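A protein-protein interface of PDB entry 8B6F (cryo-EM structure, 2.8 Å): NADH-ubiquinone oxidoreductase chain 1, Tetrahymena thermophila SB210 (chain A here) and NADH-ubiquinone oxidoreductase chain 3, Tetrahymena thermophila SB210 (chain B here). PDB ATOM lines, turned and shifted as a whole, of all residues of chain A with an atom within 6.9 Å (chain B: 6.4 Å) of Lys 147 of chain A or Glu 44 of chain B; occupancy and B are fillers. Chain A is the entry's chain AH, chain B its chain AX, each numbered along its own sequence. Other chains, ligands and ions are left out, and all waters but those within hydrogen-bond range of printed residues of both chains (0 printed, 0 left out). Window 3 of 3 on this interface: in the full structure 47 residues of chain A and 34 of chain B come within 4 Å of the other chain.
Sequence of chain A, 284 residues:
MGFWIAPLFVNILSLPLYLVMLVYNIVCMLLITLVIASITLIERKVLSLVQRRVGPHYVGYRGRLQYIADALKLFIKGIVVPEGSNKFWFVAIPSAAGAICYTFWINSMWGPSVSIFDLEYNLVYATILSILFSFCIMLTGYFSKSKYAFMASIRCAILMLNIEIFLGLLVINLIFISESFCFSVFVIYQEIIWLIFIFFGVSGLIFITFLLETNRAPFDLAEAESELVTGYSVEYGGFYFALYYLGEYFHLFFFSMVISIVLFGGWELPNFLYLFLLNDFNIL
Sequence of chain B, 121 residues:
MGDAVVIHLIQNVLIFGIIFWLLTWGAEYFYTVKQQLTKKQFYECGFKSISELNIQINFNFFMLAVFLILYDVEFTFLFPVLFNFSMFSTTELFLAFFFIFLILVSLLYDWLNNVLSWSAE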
ATOM      1  N   GLY A 141       7.771  23.156  -8.210  1.00  0.00           N
ATOM      2  CA  GLY A 141       8.279  21.888  -8.704  1.00  0.00           C
ATOM      3  C   GLY A 141       9.558  21.464  -8.011  1.00  0.00           C
ATOM      4  O   GLY A 141       9.742  20.287  -7.693  1.00  0.00           O
ATOM      5  N   SER A 144       8.855  20.558  -4.123  1.00  0.00           N
ATOM      6  CA  SER A 144       8.199  19.257  -4.098  1.00  0.00           C
ATOM      7  C   SER A 144       9.110  18.297  -4.850  1.00  0.00           C
ATOM      8  O   SER A 144       9.193  18.346  -6.081  1.00  0.00           O
ATOM      9  CB  SER A 144       6.811  19.324  -4.728  1.00  0.00           C
ATOM     10  OG  SER A 144       6.885  19.705  -6.091  1.00  0.00           O
ATOM     11  N   LYS A 145       9.789  17.426  -4.118  1.00  0.00           N
ATOM     12  CA  LYS A 145      10.892  16.661  -4.695  1.00  0.00           C
ATOM     13  C   LYS A 145      10.446  15.598  -5.663  1.00  0.00           C
ATOM     14  O   LYS A 145      11.293  14.795  -6.071  1.00  0.00           O
ATOM     15  CB  LYS A 145      11.719  16.027  -3.577  1.00  0.00           C
ATOM     16  CG  LYS A 145      12.417  17.038  -2.679  1.00  0.00           C
ATOM     17  CD  LYS A 145      13.453  17.848  -3.447  1.00  0.00           C
ATOM     18  CE  LYS A 145      14.153  18.847  -2.546  1.00  0.00           C
ATOM     19  NZ  LYS A 145      15.107  19.699  -3.309  1.00  0.00           N
ATOM     20  N   SER A 146       9.179  15.539  -6.057  1.00  0.00           N
ATOM     21  CA  SER A 146       8.767  14.588  -7.077  1.00  0.00           C
ATOM     22  C   SER A 146       9.546  14.832  -8.361  1.00  0.00           C
ATOM     23  O   SER A 146       9.685  15.971  -8.813  1.00  0.00           O
ATOM     24  CB  SER A 146       7.267  14.700  -7.338  1.00  0.00           C
ATOM     25  OG  SER A 146       6.871  13.768  -8.331  1.00  0.00           O
ATOM     26  N   LYS A 147      10.064  13.751  -8.944  1.00  0.00           N
ATOM     27  CA  LYS A 147      10.793  13.871 -10.200  1.00  0.00           C
ATOM     28  C   LYS A 147       9.884  14.381 -11.310  1.00  0.00           C
ATOM     29  O   LYS A 147      10.310  15.177 -12.155  1.00  0.00           O
ATOM     30  CB  LYS A 147      11.406  12.524 -10.577  1.00  0.00           C
ATOM     31  CG  LYS A 147      12.397  11.998  -9.549  1.00  0.00           C
ATOM     32  CD  LYS A 147      12.894  10.610  -9.915  1.00  0.00           C
ATOM     33  CE  LYS A 147      13.857  10.072  -8.871  1.00  0.00           C
ATOM     34  NZ  LYS A 147      15.094  10.891  -8.781  1.00  0.00           N
ATOM     35  N   TYR A 148       8.628  13.936 -11.325  1.00  0.00           N
ATOM     36  CA  TYR A 148       7.679  14.442 -12.311  1.00  0.00           C
ATOM     37  C   TYR A 148       7.451  15.938 -12.137  1.00  0.00           C
ATOM     38  O   TYR A 148       7.394  16.683 -13.122  1.00  0.00           O
ATOM     39  CB  TYR A 148       6.358  13.683 -12.203  1.00  0.00           C
ATOM     40  CG  TYR A 148       6.488  12.203 -12.467  1.00  0.00           C
ATOM     41  CD1 TYR A 148       6.589  11.716 -13.764  1.00  0.00           C
ATOM     42  CD2 TYR A 148       6.509  11.291 -11.421  1.00  0.00           C
ATOM     43  CE1 TYR A 148       6.709  10.362 -14.012  1.00  0.00           C
ATOM     44  CE2 TYR A 148       6.629   9.936 -11.660  1.00  0.00           C
ATOM     45  CZ  TYR A 148       6.729   9.478 -12.957  1.00  0.00           C
ATOM     46  OH  TYR A 148       6.847   8.131 -13.198  1.00  0.00           O
ATOM     47  N   ALA A 149       7.312  16.396 -10.892  1.00  0.00           N
ATOM     48  CA  ALA A 149       7.141  17.823 -10.647  1.00  0.00           C
ATOM     49  C   ALA A 149       8.362  18.611 -11.095  1.00  0.00           C
ATOM     50  O   ALA A 149       8.234  19.705 -11.657  1.00  0.00           O
ATOM     51  CB  ALA A 149       6.874  18.075  -9.166  1.00  0.00           C
ATOM     52  N   PHE A 150       9.558  18.078 -10.849  1.00  0.00           N
ATOM     53  CA  PHE A 150      10.767  18.778 -11.262  1.00  0.00           C
ATOM     54  C   PHE A 150      10.869  18.846 -12.781  1.00  0.00           C
ATOM     55  O   PHE A 150      11.260  19.879 -13.333  1.00  0.00           O
ATOM     56  CB  PHE A 150      11.994  18.100 -10.654  1.00  0.00           C
ATOM     57  CG  PHE A 150      13.208  18.978 -10.609  1.00  0.00           C
ATOM     58  CD1 PHE A 150      13.131  20.266 -10.108  1.00  0.00           C
ATOM     59  CD2 PHE A 150      14.435  18.508 -11.037  1.00  0.00           C
ATOM     60  CE1 PHE A 150      14.244  21.072 -10.057  1.00  0.00           C
ATOM     61  CE2 PHE A 150      15.553  19.314 -10.987  1.00  0.00           C
ATOM     62  CZ  PHE A 150      15.457  20.595 -10.496  1.00  0.00           C
ATOM     63  N   MET A 151      10.517  17.762 -13.473  1.00  0.00           N
ATOM     64  CA  MET A 151      10.492  17.803 -14.932  1.00  0.00           C
ATOM     65  C   MET A 151       9.457  18.803 -15.429  1.00  0.00           C
ATOM     66  O   MET A 151       9.683  19.500 -16.425  1.00  0.00           O
ATOM     67  CB  MET A 151      10.212  16.411 -15.498  1.00  0.00           C
ATOM     68  CG  MET A 151      11.380  15.450 -15.347  1.00  0.00           C
ATOM     69  SD  MET A 151      11.109  13.855 -16.140  1.00  0.00           S
ATOM     70  CE  MET A 151       9.755  13.204 -15.167  1.00  0.00           C
ATOM     71  N   ALA A 152       8.318  18.895 -14.744  1.00  0.00           N
ATOM     72  CA  ALA A 152       7.320  19.900 -15.094  1.00  0.00           C
ATOM     73  C   ALA A 152       7.873  21.307 -14.918  1.00  0.00           C
ATOM     74  O   ALA A 152       7.582  22.201 -15.720  1.00  0.00           O
ATOM     75  CB  ALA A 152       6.065  19.713 -14.243  1.00  0.00           C
ATOM     76  N   SER A 153       8.665  21.527 -13.868  1.00  0.00           N
ATOM     77  CA  SER A 153       9.278  22.836 -13.670  1.00  0.00           C
ATOM     78  C   SER A 153      10.253  23.164 -14.792  1.00  0.00           C
ATOM     79  O   SER A 153      10.311  24.308 -15.257  1.00  0.00           O
ATOM     80  CB  SER A 153       9.985  22.882 -12.317  1.00  0.00           C
ATOM     81  OG  SER A 153      11.149  22.076 -12.321  1.00  0.00           O
ATOM     82  N   LEU A 228       3.234  13.533 -17.692  1.00  0.00           N
ATOM     83  CA  LEU A 228       3.530  13.575 -16.270  1.00  0.00           C
ATOM     84  C   LEU A 228       2.254  13.279 -15.495  1.00  0.00           C
ATOM     85  O   LEU A 228       1.146  13.403 -16.021  1.00  0.00           O
ATOM     86  CB  LEU A 228       4.099  14.940 -15.864  1.00  0.00           C
ATOM     87  CG  LEU A 228       5.305  15.406 -16.685  1.00  0.00           C
ATOM     88  CD1 LEU A 228       5.685  16.825 -16.320  1.00  0.00           C
ATOM     89  CD2 LEU A 228       6.487  14.475 -16.488  1.00  0.00           C
ATOM     90  N   VAL A 229       2.415  12.866 -14.237  1.00  0.00           N
ATOM     91  CA  VAL A 229       1.255  12.478 -13.439  1.00  0.00           C
ATOM     92  C   VAL A 229       0.242  13.616 -13.399  1.00  0.00           C
ATOM     93  O   VAL A 229      -0.879  13.493 -13.907  1.00  0.00           O
ATOM     94  CB  VAL A 229       1.689  12.056 -12.024  1.00  0.00           C
ATOM     95  CG1 VAL A 229       0.476  11.776 -11.145  1.00  0.00           C
ATOM     96  CG2 VAL A 229       2.588  10.831 -12.094  1.00  0.00           C
ATOM     97  N   VAL A 234       1.931  17.796  -8.516  1.00  0.00           N
ATOM     98  CA  VAL A 234       1.719  16.373  -8.280  1.00  0.00           C
ATOM     99  C   VAL A 234       1.686  16.038  -6.797  1.00  0.00           C
ATOM    100  O   VAL A 234       1.138  14.997  -6.417  1.00  0.00           O
ATOM    101  CB  VAL A 234       2.806  15.560  -9.007  1.00  0.00           C
ATOM    102  CG1 VAL A 234       4.144  15.765  -8.349  1.00  0.00           C
ATOM    103  CG2 VAL A 234       2.447  14.085  -9.021  1.00  0.00           C
ATOM    104  N   GLU A 235       2.264  16.883  -5.945  1.00  0.00           N
ATOM    105  CA  GLU A 235       2.295  16.642  -4.506  1.00  0.00           C
ATOM    106  C   GLU A 235       1.539  17.701  -3.717  1.00  0.00           C
ATOM    107  O   GLU A 235       1.705  17.779  -2.494  1.00  0.00           O
ATOM    108  CB  GLU A 235       3.742  16.561  -4.009  1.00  0.00           C
ATOM    109  CG  GLU A 235       4.445  15.274  -4.403  1.00  0.00           C
ATOM    110  CD  GLU A 235       5.883  15.230  -3.942  1.00  0.00           C
ATOM    111  OE1 GLU A 235       6.398  16.280  -3.503  1.00  0.00           O
ATOM    112  OE2 GLU A 235       6.501  14.148  -4.020  1.00  0.00           O
ATOM    113  N   PHE B  42       7.373  10.910  -0.146  1.00  0.00           N
ATOM    114  CA  PHE B  42       7.302  11.340  -1.535  1.00  0.00           C
ATOM    115  C   PHE B  42       6.480  10.358  -2.362  1.00  0.00           C
ATOM    116  O   PHE B  42       6.585   9.140  -2.199  1.00  0.00           O
ATOM    117  CB  PHE B  42       8.706  11.475  -2.122  1.00  0.00           C
ATOM    118  CG  PHE B  42       9.569  12.464  -1.399  1.00  0.00           C
ATOM    119  CD1 PHE B  42       9.202  13.797  -1.326  1.00  0.00           C
ATOM    120  CD2 PHE B  42      10.756  12.066  -0.809  1.00  0.00           C
ATOM    121  CE1 PHE B  42       9.996  14.712  -0.666  1.00  0.00           C
ATOM    122  CE2 PHE B  42      11.554  12.975  -0.147  1.00  0.00           C
ATOM    123  CZ  PHE B  42      11.174  14.301  -0.076  1.00  0.00           C
ATOM    124  N   TYR B  43       5.662  10.902  -3.258  1.00  0.00           N
ATOM    125  CA  TYR B  43       4.806  10.103  -4.124  1.00  0.00           C
ATOM    126  C   TYR B  43       5.541   9.803  -5.424  1.00  0.00           C
ATOM    127  O   TYR B  43       5.994  10.722  -6.115  1.00  0.00           O
ATOM    128  CB  TYR B  43       3.496  10.841  -4.398  1.00  0.00           C
ATOM    129  CG  TYR B  43       2.742  10.327  -5.601  1.00  0.00           C
ATOM    130  CD1 TYR B  43       1.945   9.196  -5.513  1.00  0.00           C
ATOM    131  CD2 TYR B  43       2.823  10.979  -6.822  1.00  0.00           C
ATOM    132  CE1 TYR B  43       1.252   8.726  -6.609  1.00  0.00           C
ATOM    133  CE2 TYR B  43       2.136  10.518  -7.923  1.00  0.00           C
ATOM    134  CZ  TYR B  43       1.352   9.392  -7.810  1.00  0.00           C
ATOM    135  OH  TYR B  43       0.664   8.929  -8.907  1.00  0.00           O
ATOM    136  N   GLU B  44       5.656   8.519  -5.756  1.00  0.00           N
ATOM    137  CA  GLU B  44       6.334   8.051  -6.962  1.00  0.00           C
ATOM    138  C   GLU B  44       5.487   7.000  -7.665  1.00  0.00           C
ATOM    139  O   GLU B  44       5.958   5.921  -8.029  1.00  0.00           O
ATOM    140  CB  GLU B  44       7.715   7.499  -6.626  1.00  0.00           C
ATOM    141  CG  GLU B  44       8.614   7.262  -7.832  1.00  0.00           C
ATOM    142  CD  GLU B  44       9.124   8.549  -8.449  1.00  0.00           C
ATOM    143  OE1 GLU B  44       8.766   9.635  -7.948  1.00  0.00           O
ATOM    144  OE2 GLU B  44       9.886   8.472  -9.434  1.00  0.00           O
ATOM    145  N   CYS B  45       4.201   7.302  -7.844  1.00  0.00           N
ATOM    146  CA  CYS B  45       3.270   6.418  -8.545  1.00  0.00           C
ATOM    147  C   CYS B  45       3.073   5.107  -7.785  1.00  0.00           C
ATOM    148  O   CYS B  45       3.107   4.018  -8.358  1.00  0.00           O
ATOM    149  CB  CYS B  45       3.740   6.150  -9.979  1.00  0.00           C
ATOM    150  SG  CYS B  45       3.816   7.613 -11.031  1.00  0.00           S
ATOM    151  N   GLY B  46       2.861   5.220  -6.477  1.00  0.00           N
ATOM    152  CA  GLY B  46       2.529   4.059  -5.678  1.00  0.00           C
ATOM    153  C   GLY B  46       3.701   3.221  -5.228  1.00  0.00           C
ATOM    154  O   GLY B  46       3.511   2.055  -4.874  1.00  0.00           O
ATOM    155  N   PHE B  47       4.912   3.770  -5.233  1.00  0.00           N
ATOM    156  CA  PHE B  47       6.073   3.054  -4.729  1.00  0.00           C
ATOM    157  C   PHE B  47       7.051   4.061  -4.145  1.00  0.00           C
ATOM    158  O   PHE B  47       7.008   5.251  -4.461  1.00  0.00           O
ATOM    159  CB  PHE B  47       6.738   2.213  -5.825  1.00  0.00           C
ATOM    160  CG  PHE B  47       6.027   0.919  -6.107  1.00  0.00           C
ATOM    161  CD1 PHE B  47       6.270  -0.203  -5.332  1.00  0.00           C
ATOM    162  CD2 PHE B  47       5.115   0.825  -7.144  1.00  0.00           C
ATOM    163  CE1 PHE B  47       5.618  -1.397  -5.586  1.00  0.00           C
ATOM    164  CE2 PHE B  47       4.460  -0.366  -7.405  1.00  0.00           C
ATOM    165  CZ  PHE B  47       4.712  -1.478  -6.622  1.00  0.00           C
ATOM    166  N   LYS B  48       7.929   3.570  -3.276  1.00  0.00           N
ATOM    167  CA  LYS B  48       8.861   4.453  -2.592  1.00  0.00           C
ATOM    168  C   LYS B  48       9.888   5.007  -3.572  1.00  0.00           C
ATOM    169  O   LYS B  48      10.422   4.281  -4.414  1.00  0.00           O
ATOM    170  CB  LYS B  48       9.560   3.705  -1.459  1.00  0.00           C
ATOM    171  CG  LYS B  48      10.355   4.600  -0.529  1.00  0.00           C
ATOM    172  CD  LYS B  48      10.773   3.854   0.726  1.00  0.00           C
ATOM    173  CE  LYS B  48      11.549   4.754   1.671  1.00  0.00           C
ATOM    174  NZ  LYS B  48      11.932   4.048   2.926  1.00  0.00           N
ATOM    175  N   SER B  49      10.161   6.304  -3.457  1.00  0.00           N
ATOM    176  CA  SER B  49      11.150   6.951  -4.307  1.00  0.00           C
ATOM    177  C   SER B  49      12.550   6.610  -3.815  1.00  0.00           C
ATOM    178  O   SER B  49      12.858   6.774  -2.631  1.00  0.00           O
ATOM    179  CB  SER B  49      10.942   8.465  -4.315  1.00  0.00           C
ATOM    180  OG  SER B  49      11.008   8.992  -3.003  1.00  0.00           O
ATOM    181  N   ILE B  50      13.399   6.138  -4.727  1.00  0.00           N
ATOM    182  CA  ILE B  50      14.730   5.694  -4.326  1.00  0.00           C
ATOM    183  C   ILE B  50      15.597   6.882  -3.933  1.00  0.00           C
ATOM    184  O   ILE B  50      16.355   6.816  -2.957  1.00  0.00           O
ATOM    185  CB  ILE B  50      15.382   4.855  -5.442  1.00  0.00           C
ATOM    186  CG1 ILE B  50      15.689   5.720  -6.669  1.00  0.00           C
ATOM    187  CG2 ILE B  50      14.476   3.685  -5.807  1.00  0.00           C
ATOM    188  CD1 ILE B  50      16.292   4.958  -7.825  1.00  0.00           C
ATOM    189  N   SER B  51      15.504   7.984  -4.672  1.00  0.00           N
ATOM    190  CA  SER B  51      16.373   9.135  -4.479  1.00  0.00           C
ATOM    191  C   SER B  51      15.546  10.369  -4.156  1.00  0.00           C
ATOM    192  O   SER B  51      14.498  10.604  -4.763  1.00  0.00           O
ATOM    193  CB  SER B  51      17.219   9.394  -5.731  1.00  0.00           C
ATOM    194  OG  SER B  51      18.046  10.532  -5.565  1.00  0.00           O
ATOM    195  N   GLU B  52      16.028  11.156  -3.197  1.00  0.00           N
ATOM    196  CA  GLU B  52      15.411  12.425  -2.846  1.00  0.00           C
ATOM    197  C   GLU B  52      16.504  13.443  -2.560  1.00  0.00           C
ATOM    198  O   GLU B  52      17.480  13.142  -1.869  1.00  0.00           O
ATOM    199  CB  GLU B  52      14.482  12.282  -1.635  1.00  0.00           C
ATOM    200  CG  GLU B  52      15.196  12.179  -0.294  1.00  0.00           C
ATOM    201  CD  GLU B  52      15.442  13.530   0.356  1.00  0.00           C
ATOM    202  OE1 GLU B  52      15.069  14.560  -0.243  1.00  0.00           O
ATOM    203  OE2 GLU B  52      16.007  13.561   1.468  1.00  0.00           O
ATOM    204  N   ASN B  54      18.709  14.470  -4.468  1.00  0.00           N
ATOM    205  CA  ASN B  54      19.674  14.317  -5.556  1.00  0.00           C
ATOM    206  C   ASN B  54      18.885  14.136  -6.850  1.00  0.00           C
ATOM    207  O   ASN B  54      18.766  13.036  -7.390  1.00  0.00           O
ATOM    208  CB  ASN B  54      20.613  13.148  -5.283  1.00  0.00           C
ATOM    209  CG  ASN B  54      21.838  13.166  -6.175  1.00  0.00           C
ATOM    210  OD1 ASN B  54      22.081  14.132  -6.897  1.00  0.00           O
ATOM    211  ND2 ASN B  54      22.625  12.097  -6.120  1.00  0.00           N
ATOM    212  N   ILE B  55      18.341  15.242  -7.355  1.00  0.00           N
ATOM    213  CA  ILE B  55      17.416  15.195  -8.483  1.00  0.00           C
ATOM    214  C   ILE B  55      17.969  16.013  -9.642  1.00  0.00           C
ATOM    215  O   ILE B  55      17.211  16.629 -10.398  1.00  0.00           O
ATOM    216  CB  ILE B  55      16.014  15.686  -8.076  1.00  0.00           C
ATOM    217  CG1 ILE B  55      16.096  17.083  -7.450  1.00  0.00           C
ATOM    218  CG2 ILE B  55      15.375  14.692  -7.118  1.00  0.00           C
ATOM    219  CD1 ILE B  55      14.753  17.666  -7.037  1.00  0.00           C
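Of the 15 printed residues of chain A, 8 touch a printed residue of chain B.
Hydrophobic or aromatic side chains of chain A within 4 Å of the printed part of chain B: Tyr 148, Phe 150, Val 229 and Val 234.
Of the 13 printed residues of chain B, 5 touch a printed residue of chain A.
Among the printed residues, no Asp or Glu carboxylate lies within 4 Å of a Lys or Arg side-chain nitrogen of the other chain.
Among the printed residues, merely in contact across the chains: Phe 150 of chain A with Ile 55 of chain B, Val 229 of chain A with Cys 45 of chain B, Val 229 of chain A with Tyr 43 of chain B, Lys 145 of chain A with Phe 42 of chain B, Lys 147 of chain A with Glu 44 of chain B, Val 234 of chain A with Tyr 43 of chain B, Lys 145 of chain A with Ile 55 of chain B, Glu 235 of chain A with Phe 42 of chain B and Ser 146 of chain A with Tyr 43 of chain B.
The side-chain hydroxyl (OH) of Tyr 148 of chain A sits close to the side-chain sulfur (SG) of Cys 45 of chain B (3.8 Å).
The side-chain carboxylate of Glu 235 of chain A is in hydrogen-bond range of the backbone NH of Tyr 43 of chain B, at 3.4 Å.
Ser 144 of chain A touches none of the printed residues of chain B.
Printed residues of chain B within 4 Å of Lys 147 of chain A: Glu 44.
Of the printed residues of chain B, Tyr 148 of chain A touches Cys 45 (3.7 Å).
Of the printed residues of chain A, Phe 42 of chain B touches Lys 145 (3.6 Å) and Glu 235 (3.8 Å).
Of the printed residues of chain A, Tyr 43 of chain B touches Ser 146, Val 229, Val 234 and Glu 235.
Glu 44 of chain B touches just one residue of chain A: Lys 147.
The nearest printed residue of chain B that does not touch Lys 147 of chain A is Ser 51 of chain B (4.01 Å).
The nearest printed residue of chain A that does not touch Ile 55 of chain B is Lys 147 of chain A (4.2 Å).
OG of Ser 146 of chain A sits close to N of Tyr 148 of chain A (3.5 Å).
The backbone carbonyl oxygen of Phe 150 of chain A lies within hydrogen-bond range of the side-chain hydroxyl of Ser 153 of chain A, 2.4 Å away.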
